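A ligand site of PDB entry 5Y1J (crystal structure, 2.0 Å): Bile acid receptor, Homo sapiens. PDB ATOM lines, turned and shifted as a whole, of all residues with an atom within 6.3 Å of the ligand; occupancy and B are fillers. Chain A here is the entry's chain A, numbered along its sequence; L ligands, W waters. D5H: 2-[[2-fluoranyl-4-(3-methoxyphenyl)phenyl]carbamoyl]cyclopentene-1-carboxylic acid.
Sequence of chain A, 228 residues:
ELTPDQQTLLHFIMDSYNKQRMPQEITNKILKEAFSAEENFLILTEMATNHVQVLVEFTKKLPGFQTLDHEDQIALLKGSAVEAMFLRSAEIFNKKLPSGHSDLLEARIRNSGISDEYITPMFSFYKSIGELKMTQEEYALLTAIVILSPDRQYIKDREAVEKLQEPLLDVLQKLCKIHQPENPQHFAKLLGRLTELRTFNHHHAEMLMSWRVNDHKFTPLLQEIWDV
An oxygen (O1) of the ligand is in hydrogen-bond range of the side-chain hydroxyl of Tyr 126 (2.7 Å).
O2 of the ligand sits at hydrogen-bond distance from OG of Ser 89, 3.1 Å away.
ND1 of His 51 lies within hydrogen-bond range of O of Met 47, 3.1 Å away.
The side-chain hydroxyl of Ser 89 sits at hydrogen-bond distance from the backbone carbonyl oxygen of Met 85.
OG1 of Thr 45 is in hydrogen-bond range of O of Phe 41 (2.9 Å).
A ring nitrogen (ND1) of His 51 sits close to a fluorine (F) of the ligand.
CD1 of Leu 44 touches C8 of the ligand, 3.6 Å away.
N of Thr 45 touches C of the ligand, 3.8 Å away.
Met 47 touches the ligand.
Ala 48 touches the ligand (CB to C6, 3.9 Å).
Met 85 touches the ligand.
Phe 86 touches the ligand (CE1 to C12, 3.98 Å).
CD1 of Ile 92 touches O3 of the ligand (3.5 Å).
Phe 93 touches the ligand (CB to C17, 3.9 Å).
Leu 105 touches the ligand (CD2 to C17, 3.8 Å).
CD1 of Ile 109 touches O1 of the ligand (3.5 Å).
Met 122 touches the ligand.
His 204 touches the ligand (CD2 to C3, 3.6 Å).
CE of Met 207 touches C4 of the ligand, at 3.8 Å.
Leu 208 touches the ligand (CD1 to C2, 3.8 Å).
Trp 211 touches the ligand.
CE2 of Phe 218 touches O of the ligand, 3.5 Å away.
Trp 226 touches the ligand.
Of the 28 residues printed, 20 come within 4 Å of the ligand.
Water W1 lies within hydrogen-bond range of an oxygen (O3) of the ligand and the side-chain sulfur (SD) of Met 22.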
ATOM      1  N   MET A  22     -30.269 -31.129 -14.063  1.00  0.00           N
ATOM      2  CA  MET A  22     -29.225 -30.204 -14.354  1.00  0.00           C
ATOM      3  C   MET A  22     -29.689 -29.732 -15.727  1.00  0.00           C
ATOM      4  O   MET A  22     -29.483 -30.428 -16.704  1.00  0.00           O
ATOM      5  CB  MET A  22     -27.893 -30.953 -14.372  1.00  0.00           C
ATOM      6  CG  MET A  22     -26.754 -30.121 -14.915  1.00  0.00           C
ATOM      7  SD  MET A  22     -26.797 -28.405 -14.342  1.00  0.00           S
ATOM      8  CE  MET A  22     -25.011 -28.160 -14.369  1.00  0.00           C
ATOM      9  N   PHE A  41     -18.449 -16.864 -13.915  1.00  0.00           N
ATOM     10  CA  PHE A  41     -19.332 -16.454 -12.850  1.00  0.00           C
ATOM     11  C   PHE A  41     -20.772 -16.443 -13.292  1.00  0.00           C
ATOM     12  O   PHE A  41     -21.654 -16.716 -12.457  1.00  0.00           O
ATOM     13  CB  PHE A  41     -18.909 -15.082 -12.318  1.00  0.00           C
ATOM     14  CG  PHE A  41     -19.775 -14.571 -11.230  1.00  0.00           C
ATOM     15  CD1 PHE A  41     -19.596 -15.037  -9.921  1.00  0.00           C
ATOM     16  CD2 PHE A  41     -20.701 -13.602 -11.488  1.00  0.00           C
ATOM     17  CE1 PHE A  41     -20.431 -14.547  -8.868  1.00  0.00           C
ATOM     18  CE2 PHE A  41     -21.496 -13.075 -10.473  1.00  0.00           C
ATOM     19  CZ  PHE A  41     -21.360 -13.555  -9.164  1.00  0.00           C
ATOM     20  N   LEU A  44     -21.715 -20.046 -13.133  1.00  0.00           N
ATOM     21  CA  LEU A  44     -21.857 -20.388 -11.729  1.00  0.00           C
ATOM     22  C   LEU A  44     -23.175 -19.873 -11.058  1.00  0.00           C
ATOM     23  O   LEU A  44     -23.832 -20.597 -10.271  1.00  0.00           O
ATOM     24  CB  LEU A  44     -20.606 -19.982 -10.965  1.00  0.00           C
ATOM     25  CG  LEU A  44     -20.387 -20.688  -9.630  1.00  0.00           C
ATOM     26  CD1 LEU A  44     -20.157 -22.209  -9.731  1.00  0.00           C
ATOM     27  CD2 LEU A  44     -19.198 -20.055  -8.855  1.00  0.00           C
ATOM     28  N   THR A  45     -23.578 -18.665 -11.445  1.00  0.00           N
ATOM     29  CA  THR A  45     -24.808 -18.019 -11.062  1.00  0.00           C
ATOM     30  C   THR A  45     -25.973 -18.872 -11.484  1.00  0.00           C
ATOM     31  O   THR A  45     -26.885 -19.112 -10.671  1.00  0.00           O
ATOM     32  CB  THR A  45     -24.891 -16.565 -11.601  1.00  0.00           C
ATOM     33  OG1 THR A  45     -23.940 -15.795 -10.909  1.00  0.00           O
ATOM     34  CG2 THR A  45     -26.199 -15.964 -11.409  1.00  0.00           C
ATOM     35  N   GLU A  46     -25.997 -19.321 -12.735  1.00  0.00           N
ATOM     36  CA  GLU A  46     -27.023 -20.161 -13.237  1.00  0.00           C
ATOM     37  C   GLU A  46     -27.070 -21.475 -12.468  1.00  0.00           C
ATOM     38  O   GLU A  46     -28.156 -21.935 -12.152  1.00  0.00           O
ATOM     39  CB  GLU A  46     -26.934 -20.397 -14.767  1.00  0.00           C
ATOM     40  CG  GLU A  46     -26.997 -19.071 -15.538  1.00  0.00           C
ATOM     41  CD  GLU A  46     -27.098 -19.212 -17.080  1.00  0.00           C
ATOM     42  OE1 GLU A  46     -27.306 -20.333 -17.581  1.00  0.00           O
ATOM     43  OE2 GLU A  46     -27.035 -18.173 -17.794  1.00  0.00           O
ATOM     44  N   MET A  47     -25.925 -22.048 -12.182  1.00  0.00           N
ATOM     45  CA  MET A  47     -25.861 -23.299 -11.443  1.00  0.00           C
ATOM     46  C   MET A  47     -26.436 -23.141 -10.010  1.00  0.00           C
ATOM     47  O   MET A  47     -27.235 -23.973  -9.549  1.00  0.00           O
ATOM     48  CB  MET A  47     -24.445 -23.824 -11.339  1.00  0.00           C
ATOM     49  CG  MET A  47     -23.876 -24.344 -12.663  1.00  0.00           C
ATOM     50  SD  MET A  47     -22.063 -24.501 -12.640  1.00  0.00           S
ATOM     51  CE  MET A  47     -21.715 -25.767 -11.413  1.00  0.00           C
ATOM     52  N   ALA A  48     -25.976 -22.113  -9.328  1.00  0.00           N
ATOM     53  CA  ALA A  48     -26.497 -21.837  -8.006  1.00  0.00           C
ATOM     54  C   ALA A  48     -27.998 -21.589  -8.046  1.00  0.00           C
ATOM     55  O   ALA A  48     -28.718 -22.166  -7.239  1.00  0.00           O
ATOM     56  CB  ALA A  48     -25.739 -20.730  -7.309  1.00  0.00           C
ATOM     57  N   HIS A  51     -29.794 -24.895  -8.309  1.00  0.00           N
ATOM     58  CA  HIS A  51     -29.730 -25.591  -7.015  1.00  0.00           C
ATOM     59  C   HIS A  51     -30.792 -25.054  -6.075  1.00  0.00           C
ATOM     60  O   HIS A  51     -31.436 -25.817  -5.402  1.00  0.00           O
ATOM     61  CB  HIS A  51     -28.408 -25.417  -6.350  1.00  0.00           C
ATOM     62  CG  HIS A  51     -27.356 -26.362  -6.818  1.00  0.00           C
ATOM     63  ND1 HIS A  51     -26.172 -25.940  -7.444  1.00  0.00           N
ATOM     64  CD2 HIS A  51     -27.271 -27.708  -6.705  1.00  0.00           C
ATOM     65  CE1 HIS A  51     -25.431 -26.991  -7.717  1.00  0.00           C
ATOM     66  NE2 HIS A  51     -26.082 -28.068  -7.325  1.00  0.00           N
ATOM     67  N   MET A  85     -26.959 -27.131  -1.096  1.00  0.00           N
ATOM     68  CA  MET A  85     -26.239 -26.905  -2.328  1.00  0.00           C
ATOM     69  C   MET A  85     -24.901 -27.683  -2.407  1.00  0.00           C
ATOM     70  O   MET A  85     -24.621 -28.316  -3.417  1.00  0.00           O
ATOM     71  CB  MET A  85     -25.962 -25.390  -2.528  1.00  0.00           C
ATOM     72  CG  MET A  85     -25.241 -25.156  -3.858  1.00  0.00           C
ATOM     73  SD  MET A  85     -25.193 -23.444  -4.327  1.00  0.00           S
ATOM     74  CE  MET A  85     -23.919 -22.816  -3.265  1.00  0.00           C
ATOM     75  N   PHE A  86     -24.039 -27.533  -1.410  1.00  0.00           N
ATOM     76  CA  PHE A  86     -22.770 -28.233  -1.440  1.00  0.00           C
ATOM     77  C   PHE A  86     -22.907 -29.712  -1.329  1.00  0.00           C
ATOM     78  O   PHE A  86     -22.087 -30.407  -1.851  1.00  0.00           O
ATOM     79  CB  PHE A  86     -21.820 -27.692  -0.421  1.00  0.00           C
ATOM     80  CG  PHE A  86     -21.290 -26.322  -0.759  1.00  0.00           C
ATOM     81  CD1 PHE A  86     -20.625 -26.099  -1.967  1.00  0.00           C
ATOM     82  CD2 PHE A  86     -21.460 -25.266   0.099  1.00  0.00           C
ATOM     83  CE1 PHE A  86     -20.127 -24.823  -2.271  1.00  0.00           C
ATOM     84  CE2 PHE A  86     -20.939 -24.009  -0.193  1.00  0.00           C
ATOM     85  CZ  PHE A  86     -20.309 -23.777  -1.397  1.00  0.00           C
ATOM     86  N   ARG A  88     -25.478 -31.481  -2.777  1.00  0.00           N
ATOM     87  CA  ARG A  88     -25.839 -31.824  -4.087  1.00  0.00           C
ATOM     88  C   ARG A  88     -24.609 -31.744  -5.075  1.00  0.00           C
ATOM     89  O   ARG A  88     -24.401 -32.627  -5.889  1.00  0.00           O
ATOM     90  CB  ARG A  88     -26.987 -30.896  -4.502  1.00  0.00           C
ATOM     91  CG  ARG A  88     -27.491 -31.131  -5.901  1.00  0.00           C
ATOM     92  CD  ARG A  88     -29.034 -31.025  -5.941  1.00  0.00           C
ATOM     93  NE  ARG A  88     -29.518 -32.330  -6.373  1.00  0.00           N
ATOM     94  CZ  ARG A  88     -30.682 -32.913  -6.093  1.00  0.00           C
ATOM     95  NH1 ARG A  88     -31.580 -32.394  -5.240  1.00  0.00           N
ATOM     96  NH2 ARG A  88     -30.905 -34.095  -6.659  1.00  0.00           N
ATOM     97  N   SER A  89     -23.803 -30.718  -4.951  1.00  0.00           N
ATOM     98  CA  SER A  89     -22.519 -30.608  -5.693  1.00  0.00           C
ATOM     99  C   SER A  89     -21.608 -31.780  -5.427  1.00  0.00           C
ATOM    100  O   SER A  89     -21.050 -32.320  -6.370  1.00  0.00           O
ATOM    101  CB  SER A  89     -21.831 -29.284  -5.387  1.00  0.00           C
ATOM    102  OG  SER A  89     -22.684 -28.188  -5.760  1.00  0.00           O
ATOM    103  N   ALA A  90     -21.498 -32.216  -4.168  1.00  0.00           N
ATOM    104  CA  ALA A  90     -20.713 -33.391  -3.838  1.00  0.00           C
ATOM    105  C   ALA A  90     -21.260 -34.654  -4.527  1.00  0.00           C
ATOM    106  O   ALA A  90     -20.466 -35.403  -5.132  1.00  0.00           O
ATOM    107  CB  ALA A  90     -20.631 -33.586  -2.342  1.00  0.00           C
ATOM    108  N   ILE A  92     -22.939 -34.837  -7.297  1.00  0.00           N
ATOM    109  CA  ILE A  92     -22.684 -34.669  -8.726  1.00  0.00           C
ATOM    110  C   ILE A  92     -21.252 -34.902  -9.063  1.00  0.00           C
ATOM    111  O   ILE A  92     -20.992 -35.688  -9.997  1.00  0.00           O
ATOM    112  CB  ILE A  92     -23.171 -33.326  -9.253  1.00  0.00           C
ATOM    113  CG1 ILE A  92     -24.684 -33.304  -9.188  1.00  0.00           C
ATOM    114  CG2 ILE A  92     -22.641 -33.103 -10.693  1.00  0.00           C
ATOM    115  CD1 ILE A  92     -25.300 -31.935  -9.321  1.00  0.00           C
ATOM    116  N   PHE A  93     -20.346 -34.258  -8.328  1.00  0.00           N
ATOM    117  CA  PHE A  93     -18.911 -34.406  -8.471  1.00  0.00           C
ATOM    118  C   PHE A  93     -18.494 -35.879  -8.393  1.00  0.00           C
ATOM    119  O   PHE A  93     -17.661 -36.359  -9.144  1.00  0.00           O
ATOM    120  CB  PHE A  93     -18.145 -33.548  -7.459  1.00  0.00           C
ATOM    121  CG  PHE A  93     -16.614 -33.610  -7.608  1.00  0.00           C
ATOM    122  CD1 PHE A  93     -15.933 -32.781  -8.499  1.00  0.00           C
ATOM    123  CD2 PHE A  93     -15.884 -34.474  -6.821  1.00  0.00           C
ATOM    124  CE1 PHE A  93     -14.538 -32.853  -8.602  1.00  0.00           C
ATOM    125  CE2 PHE A  93     -14.466 -34.584  -6.938  1.00  0.00           C
ATOM    126  CZ  PHE A  93     -13.819 -33.761  -7.809  1.00  0.00           C
ATOM    127  N   SER A 102     -15.799 -32.873 -16.071  1.00  0.00           N
ATOM    128  CA  SER A 102     -15.471 -32.511 -14.709  1.00  0.00           C
ATOM    129  C   SER A 102     -14.311 -31.536 -14.619  1.00  0.00           C
ATOM    130  O   SER A 102     -14.358 -30.563 -13.840  1.00  0.00           O
ATOM    131  CB  SER A 102     -15.154 -33.732 -13.888  1.00  0.00           C
ATOM    132  OG  SER A 102     -15.012 -33.339 -12.533  1.00  0.00           O
ATOM    133  N   LEU A 105     -15.576 -28.052 -15.945  1.00  0.00           N
ATOM    134  CA  LEU A 105     -16.362 -27.404 -14.895  1.00  0.00           C
ATOM    135  C   LEU A 105     -15.509 -26.914 -13.697  1.00  0.00           C
ATOM    136  O   LEU A 105     -15.574 -25.745 -13.308  1.00  0.00           O
ATOM    137  CB  LEU A 105     -17.382 -28.376 -14.356  1.00  0.00           C
ATOM    138  CG  LEU A 105     -18.301 -27.734 -13.294  1.00  0.00           C
ATOM    139  CD1 LEU A 105     -18.881 -26.355 -13.645  1.00  0.00           C
ATOM    140  CD2 LEU A 105     -19.441 -28.709 -13.004  1.00  0.00           C
ATOM    141  N   ILE A 109     -14.998 -23.082 -12.252  1.00  0.00           N
ATOM    142  CA  ILE A 109     -15.314 -22.704 -10.844  1.00  0.00           C
ATOM    143  C   ILE A 109     -14.096 -22.017 -10.225  1.00  0.00           C
ATOM    144  O   ILE A 109     -14.234 -21.014  -9.532  1.00  0.00           O
ATOM    145  CB  ILE A 109     -15.734 -23.918 -10.039  1.00  0.00           C
ATOM    146  CG1 ILE A 109     -17.077 -24.429 -10.571  1.00  0.00           C
ATOM    147  CG2 ILE A 109     -15.835 -23.548  -8.585  1.00  0.00           C
ATOM    148  CD1 ILE A 109     -17.460 -25.801  -9.958  1.00  0.00           C
ATOM    149  N   MET A 122     -13.976 -26.477  -1.168  1.00  0.00           N
ATOM    150  CA  MET A 122     -15.124 -27.193  -1.738  1.00  0.00           C
ATOM    151  C   MET A 122     -14.703 -28.539  -2.300  1.00  0.00           C
ATOM    152  O   MET A 122     -15.291 -29.579  -1.969  1.00  0.00           O
ATOM    153  CB  MET A 122     -15.756 -26.331  -2.843  1.00  0.00           C
ATOM    154  CG  MET A 122     -16.291 -24.974  -2.354  1.00  0.00           C
ATOM    155  SD  MET A 122     -16.662 -23.856  -3.731  1.00  0.00           S
ATOM    156  CE  MET A 122     -16.716 -24.925  -5.162  1.00  0.00           C
ATOM    157  N   PHE A 123     -13.655 -28.534  -3.142  1.00  0.00           N
ATOM    158  CA  PHE A 123     -13.227 -29.774  -3.757  1.00  0.00           C
ATOM    159  C   PHE A 123     -12.620 -30.770  -2.801  1.00  0.00           C
ATOM    160  O   PHE A 123     -12.880 -31.964  -2.970  1.00  0.00           O
ATOM    161  CB  PHE A 123     -12.315 -29.486  -4.961  1.00  0.00           C
ATOM    162  CG  PHE A 123     -13.069 -28.932  -6.117  1.00  0.00           C
ATOM    163  CD1 PHE A 123     -13.695 -29.792  -7.030  1.00  0.00           C
ATOM    164  CD2 PHE A 123     -13.299 -27.587  -6.220  1.00  0.00           C
ATOM    165  CE1 PHE A 123     -14.420 -29.308  -8.081  1.00  0.00           C
ATOM    166  CE2 PHE A 123     -14.054 -27.098  -7.279  1.00  0.00           C
ATOM    167  CZ  PHE A 123     -14.610 -27.956  -8.191  1.00  0.00           C
ATOM    168  N   TYR A 126     -15.732 -32.359  -1.512  1.00  0.00           N
ATOM    169  CA  TYR A 126     -16.304 -33.334  -2.431  1.00  0.00           C
ATOM    170  C   TYR A 126     -15.551 -34.713  -2.368  1.00  0.00           C
ATOM    171  O   TYR A 126     -16.183 -35.783  -2.347  1.00  0.00           O
ATOM    172  CB  TYR A 126     -16.313 -32.798  -3.846  1.00  0.00           C
ATOM    173  CG  TYR A 126     -17.038 -31.456  -4.015  1.00  0.00           C
ATOM    174  CD1 TYR A 126     -18.063 -31.079  -3.146  1.00  0.00           C
ATOM    175  CD2 TYR A 126     -16.706 -30.600  -5.055  1.00  0.00           C
ATOM    176  CE1 TYR A 126     -18.721 -29.871  -3.304  1.00  0.00           C
ATOM    177  CE2 TYR A 126     -17.326 -29.353  -5.195  1.00  0.00           C
ATOM    178  CZ  TYR A 126     -18.399 -29.023  -4.364  1.00  0.00           C
ATOM    179  OH  TYR A 126     -19.033 -27.808  -4.479  1.00  0.00           O
ATOM    180  N   HIS A 204     -18.961 -19.975   2.847  1.00  0.00           N
ATOM    181  CA  HIS A 204     -19.805 -19.365   1.816  1.00  0.00           C
ATOM    182  C   HIS A 204     -19.959 -17.870   2.019  1.00  0.00           C
ATOM    183  O   HIS A 204     -19.895 -17.140   1.060  1.00  0.00           O
ATOM    184  CB  HIS A 204     -21.152 -20.077   1.776  1.00  0.00           C
ATOM    185  CG  HIS A 204     -22.092 -19.576   0.744  1.00  0.00           C
ATOM    186  ND1 HIS A 204     -22.950 -18.517   0.978  1.00  0.00           N
ATOM    187  CD2 HIS A 204     -22.349 -19.994  -0.513  1.00  0.00           C
ATOM    188  CE1 HIS A 204     -23.728 -18.349  -0.068  1.00  0.00           C
ATOM    189  NE2 HIS A 204     -23.353 -19.210  -1.011  1.00  0.00           N
ATOM    190  N   MET A 207     -16.900 -16.201   0.785  1.00  0.00           N
ATOM    191  CA  MET A 207     -16.958 -16.191  -0.692  1.00  0.00           C
ATOM    192  C   MET A 207     -17.760 -15.027  -1.257  1.00  0.00           C
ATOM    193  O   MET A 207     -17.287 -14.294  -2.134  1.00  0.00           O
ATOM    194  CB  MET A 207     -17.471 -17.532  -1.327  1.00  0.00           C
ATOM    195  CG  MET A 207     -16.654 -18.788  -0.909  1.00  0.00           C
ATOM    196  SD  MET A 207     -17.475 -20.310  -1.391  1.00  0.00           S
ATOM    197  CE  MET A 207     -17.368 -20.229  -3.167  1.00  0.00           C
ATOM    198  N   LEU A 208     -18.972 -14.829  -0.713  1.00  0.00           N
ATOM    199  CA  LEU A 208     -19.839 -13.773  -1.143  1.00  0.00           C
ATOM    200  C   LEU A 208     -19.206 -12.407  -0.920  1.00  0.00           C
ATOM    201  O   LEU A 208     -19.266 -11.539  -1.783  1.00  0.00           O
ATOM    202  CB  LEU A 208     -21.169 -13.825  -0.400  1.00  0.00           C
ATOM    203  CG  LEU A 208     -22.325 -14.550  -1.047  1.00  0.00           C
ATOM    204  CD1 LEU A 208     -22.029 -15.796  -1.814  1.00  0.00           C
ATOM    205  CD2 LEU A 208     -23.521 -14.759  -0.087  1.00  0.00           C
ATOM    206  N   TRP A 211     -16.463 -11.889  -3.580  1.00  0.00           N
ATOM    207  CA  TRP A 211     -17.105 -11.535  -4.794  1.00  0.00           C
ATOM    208  C   TRP A 211     -17.574 -10.078  -4.866  1.00  0.00           C
ATOM    209  O   TRP A 211     -17.460  -9.388  -5.935  1.00  0.00           O
ATOM    210  CB  TRP A 211     -18.258 -12.465  -5.141  1.00  0.00           C
ATOM    211  CG  TRP A 211     -17.855 -13.612  -6.052  1.00  0.00           C
ATOM    212  CD1 TRP A 211     -17.253 -13.510  -7.289  1.00  0.00           C
ATOM    213  CD2 TRP A 211     -18.087 -15.034  -5.845  1.00  0.00           C
ATOM    214  NE1 TRP A 211     -17.040 -14.782  -7.821  1.00  0.00           N
ATOM    215  CE2 TRP A 211     -17.543 -15.720  -6.943  1.00  0.00           C
ATOM    216  CE3 TRP A 211     -18.700 -15.773  -4.805  1.00  0.00           C
ATOM    217  CZ2 TRP A 211     -17.608 -17.125  -7.069  1.00  0.00           C
ATOM    218  CZ3 TRP A 211     -18.797 -17.120  -4.905  1.00  0.00           C
ATOM    219  CH2 TRP A 211     -18.218 -17.819  -6.048  1.00  0.00           C
ATOM    220  N   PHE A 218     -25.104 -10.336  -7.549  1.00  0.00           N
ATOM    221  CA  PHE A 218     -25.897 -11.540  -7.508  1.00  0.00           C
ATOM    222  C   PHE A 218     -27.299 -11.285  -7.964  1.00  0.00           C
ATOM    223  O   PHE A 218     -27.881 -10.218  -7.693  1.00  0.00           O
ATOM    224  CB  PHE A 218     -25.867 -12.137  -6.097  1.00  0.00           C
ATOM    225  CG  PHE A 218     -24.521 -12.617  -5.715  1.00  0.00           C
ATOM    226  CD1 PHE A 218     -23.613 -11.758  -5.128  1.00  0.00           C
ATOM    227  CD2 PHE A 218     -24.134 -13.925  -6.020  1.00  0.00           C
ATOM    228  CE1 PHE A 218     -22.328 -12.189  -4.833  1.00  0.00           C
ATOM    229  CE2 PHE A 218     -22.879 -14.342  -5.773  1.00  0.00           C
ATOM    230  CZ  PHE A 218     -21.961 -13.475  -5.184  1.00  0.00           C
ATOM    231  N   LEU A 222     -30.627 -15.492  -5.710  1.00  0.00           N
ATOM    232  CA  LEU A 222     -29.463 -15.626  -4.814  1.00  0.00           C
ATOM    233  C   LEU A 222     -29.407 -14.553  -3.761  1.00  0.00           C
ATOM    234  O   LEU A 222     -29.079 -14.799  -2.587  1.00  0.00           O
ATOM    235  CB  LEU A 222     -28.170 -15.661  -5.691  1.00  0.00           C
ATOM    236  CG  LEU A 222     -28.182 -16.756  -6.754  1.00  0.00           C
ATOM    237  CD1 LEU A 222     -26.856 -16.904  -7.512  1.00  0.00           C
ATOM    238  CD2 LEU A 222     -28.511 -18.138  -6.255  1.00  0.00           C
ATOM    239  N   TRP A 226     -29.683 -15.963   0.170  1.00  0.00           N
ATOM    240  CA  TRP A 226     -28.459 -15.886   0.958  1.00  0.00           C
ATOM    241  C   TRP A 226     -28.386 -14.546   1.684  1.00  0.00           C
ATOM    242  O   TRP A 226     -27.371 -14.224   2.192  1.00  0.00           O
ATOM    243  CB  TRP A 226     -27.244 -15.930   0.044  1.00  0.00           C
ATOM    244  CG  TRP A 226     -27.080 -17.262  -0.614  1.00  0.00           C
ATOM    245  CD1 TRP A 226     -27.520 -18.455  -0.181  1.00  0.00           C
ATOM    246  CD2 TRP A 226     -26.439 -17.499  -1.858  1.00  0.00           C
ATOM    247  NE1 TRP A 226     -27.174 -19.454  -1.059  1.00  0.00           N
ATOM    248  CE2 TRP A 226     -26.481 -18.912  -2.087  1.00  0.00           C
ATOM    249  CE3 TRP A 226     -25.726 -16.685  -2.759  1.00  0.00           C
ATOM    250  CZ2 TRP A 226     -25.953 -19.512  -3.225  1.00  0.00           C
ATOM    251  CZ3 TRP A 226     -25.146 -17.305  -3.894  1.00  0.00           C
ATOM    252  CH2 TRP A 226     -25.254 -18.694  -4.110  1.00  0.00           C
HETATM  253  F   D5H L   1     -23.052 -24.669  -8.200  1.00  0.00           F
HETATM  254  C9  D5H L   1     -22.117 -24.198  -7.474  1.00  0.00           C
HETATM  255  C8  D5H L   1     -22.236 -22.957  -6.931  1.00  0.00           C
HETATM  256  C7  D5H L   1     -21.286 -22.404  -6.132  1.00  0.00           C
HETATM  257  C5  D5H L   1     -21.438 -21.034  -5.562  1.00  0.00           C
HETATM  258  C4  D5H L   1     -20.948 -20.721  -4.342  1.00  0.00           C
HETATM  259  C3  D5H L   1     -21.077 -19.487  -3.819  1.00  0.00           C
HETATM  260  C2  D5H L   1     -21.645 -18.478  -4.519  1.00  0.00           C
HETATM  261  C1  D5H L   1     -22.135 -18.738  -5.763  1.00  0.00           C
HETATM  262  O   D5H L   1     -22.743 -17.749  -6.457  1.00  0.00           O
HETATM  263  C   D5H L   1     -22.786 -17.730  -7.845  1.00  0.00           C
HETATM  264  C6  D5H L   1     -22.026 -20.019  -6.275  1.00  0.00           C
HETATM  265  C12 D5H L   1     -20.155 -23.168  -5.895  1.00  0.00           C
HETATM  266  C11 D5H L   1     -19.992 -24.412  -6.422  1.00  0.00           C
HETATM  267  C10 D5H L   1     -20.937 -25.008  -7.208  1.00  0.00           C
HETATM  268  N   D5H L   1     -20.894 -26.214  -7.789  1.00  0.00           N
HETATM  269  C13 D5H L   1     -19.972 -27.138  -7.725  1.00  0.00           C
HETATM  270  O1  D5H L   1     -19.000 -26.964  -7.077  1.00  0.00           O
HETATM  271  C14 D5H L   1     -20.041 -28.397  -8.477  1.00  0.00           C
HETATM  272  C15 D5H L   1     -21.041 -28.995  -9.076  1.00  0.00           C
HETATM  273  C19 D5H L   1     -22.400 -28.522  -9.239  1.00  0.00           C
HETATM  274  O3  D5H L   1     -23.188 -29.178  -9.976  1.00  0.00           O
HETATM  275  O2  D5H L   1     -22.870 -27.571  -8.755  1.00  0.00           O
HETATM  276  C18 D5H L   1     -18.787 -29.218  -8.614  1.00  0.00           C
HETATM  277  C17 D5H L   1     -19.152 -30.342  -9.530  1.00  0.00           C
HETATM  278  C16 D5H L   1     -20.661 -30.327  -9.623  1.00  0.00           C
HETATM  279  O   HOH W   1     -25.693 -28.701 -10.906  1.00  0.00           O
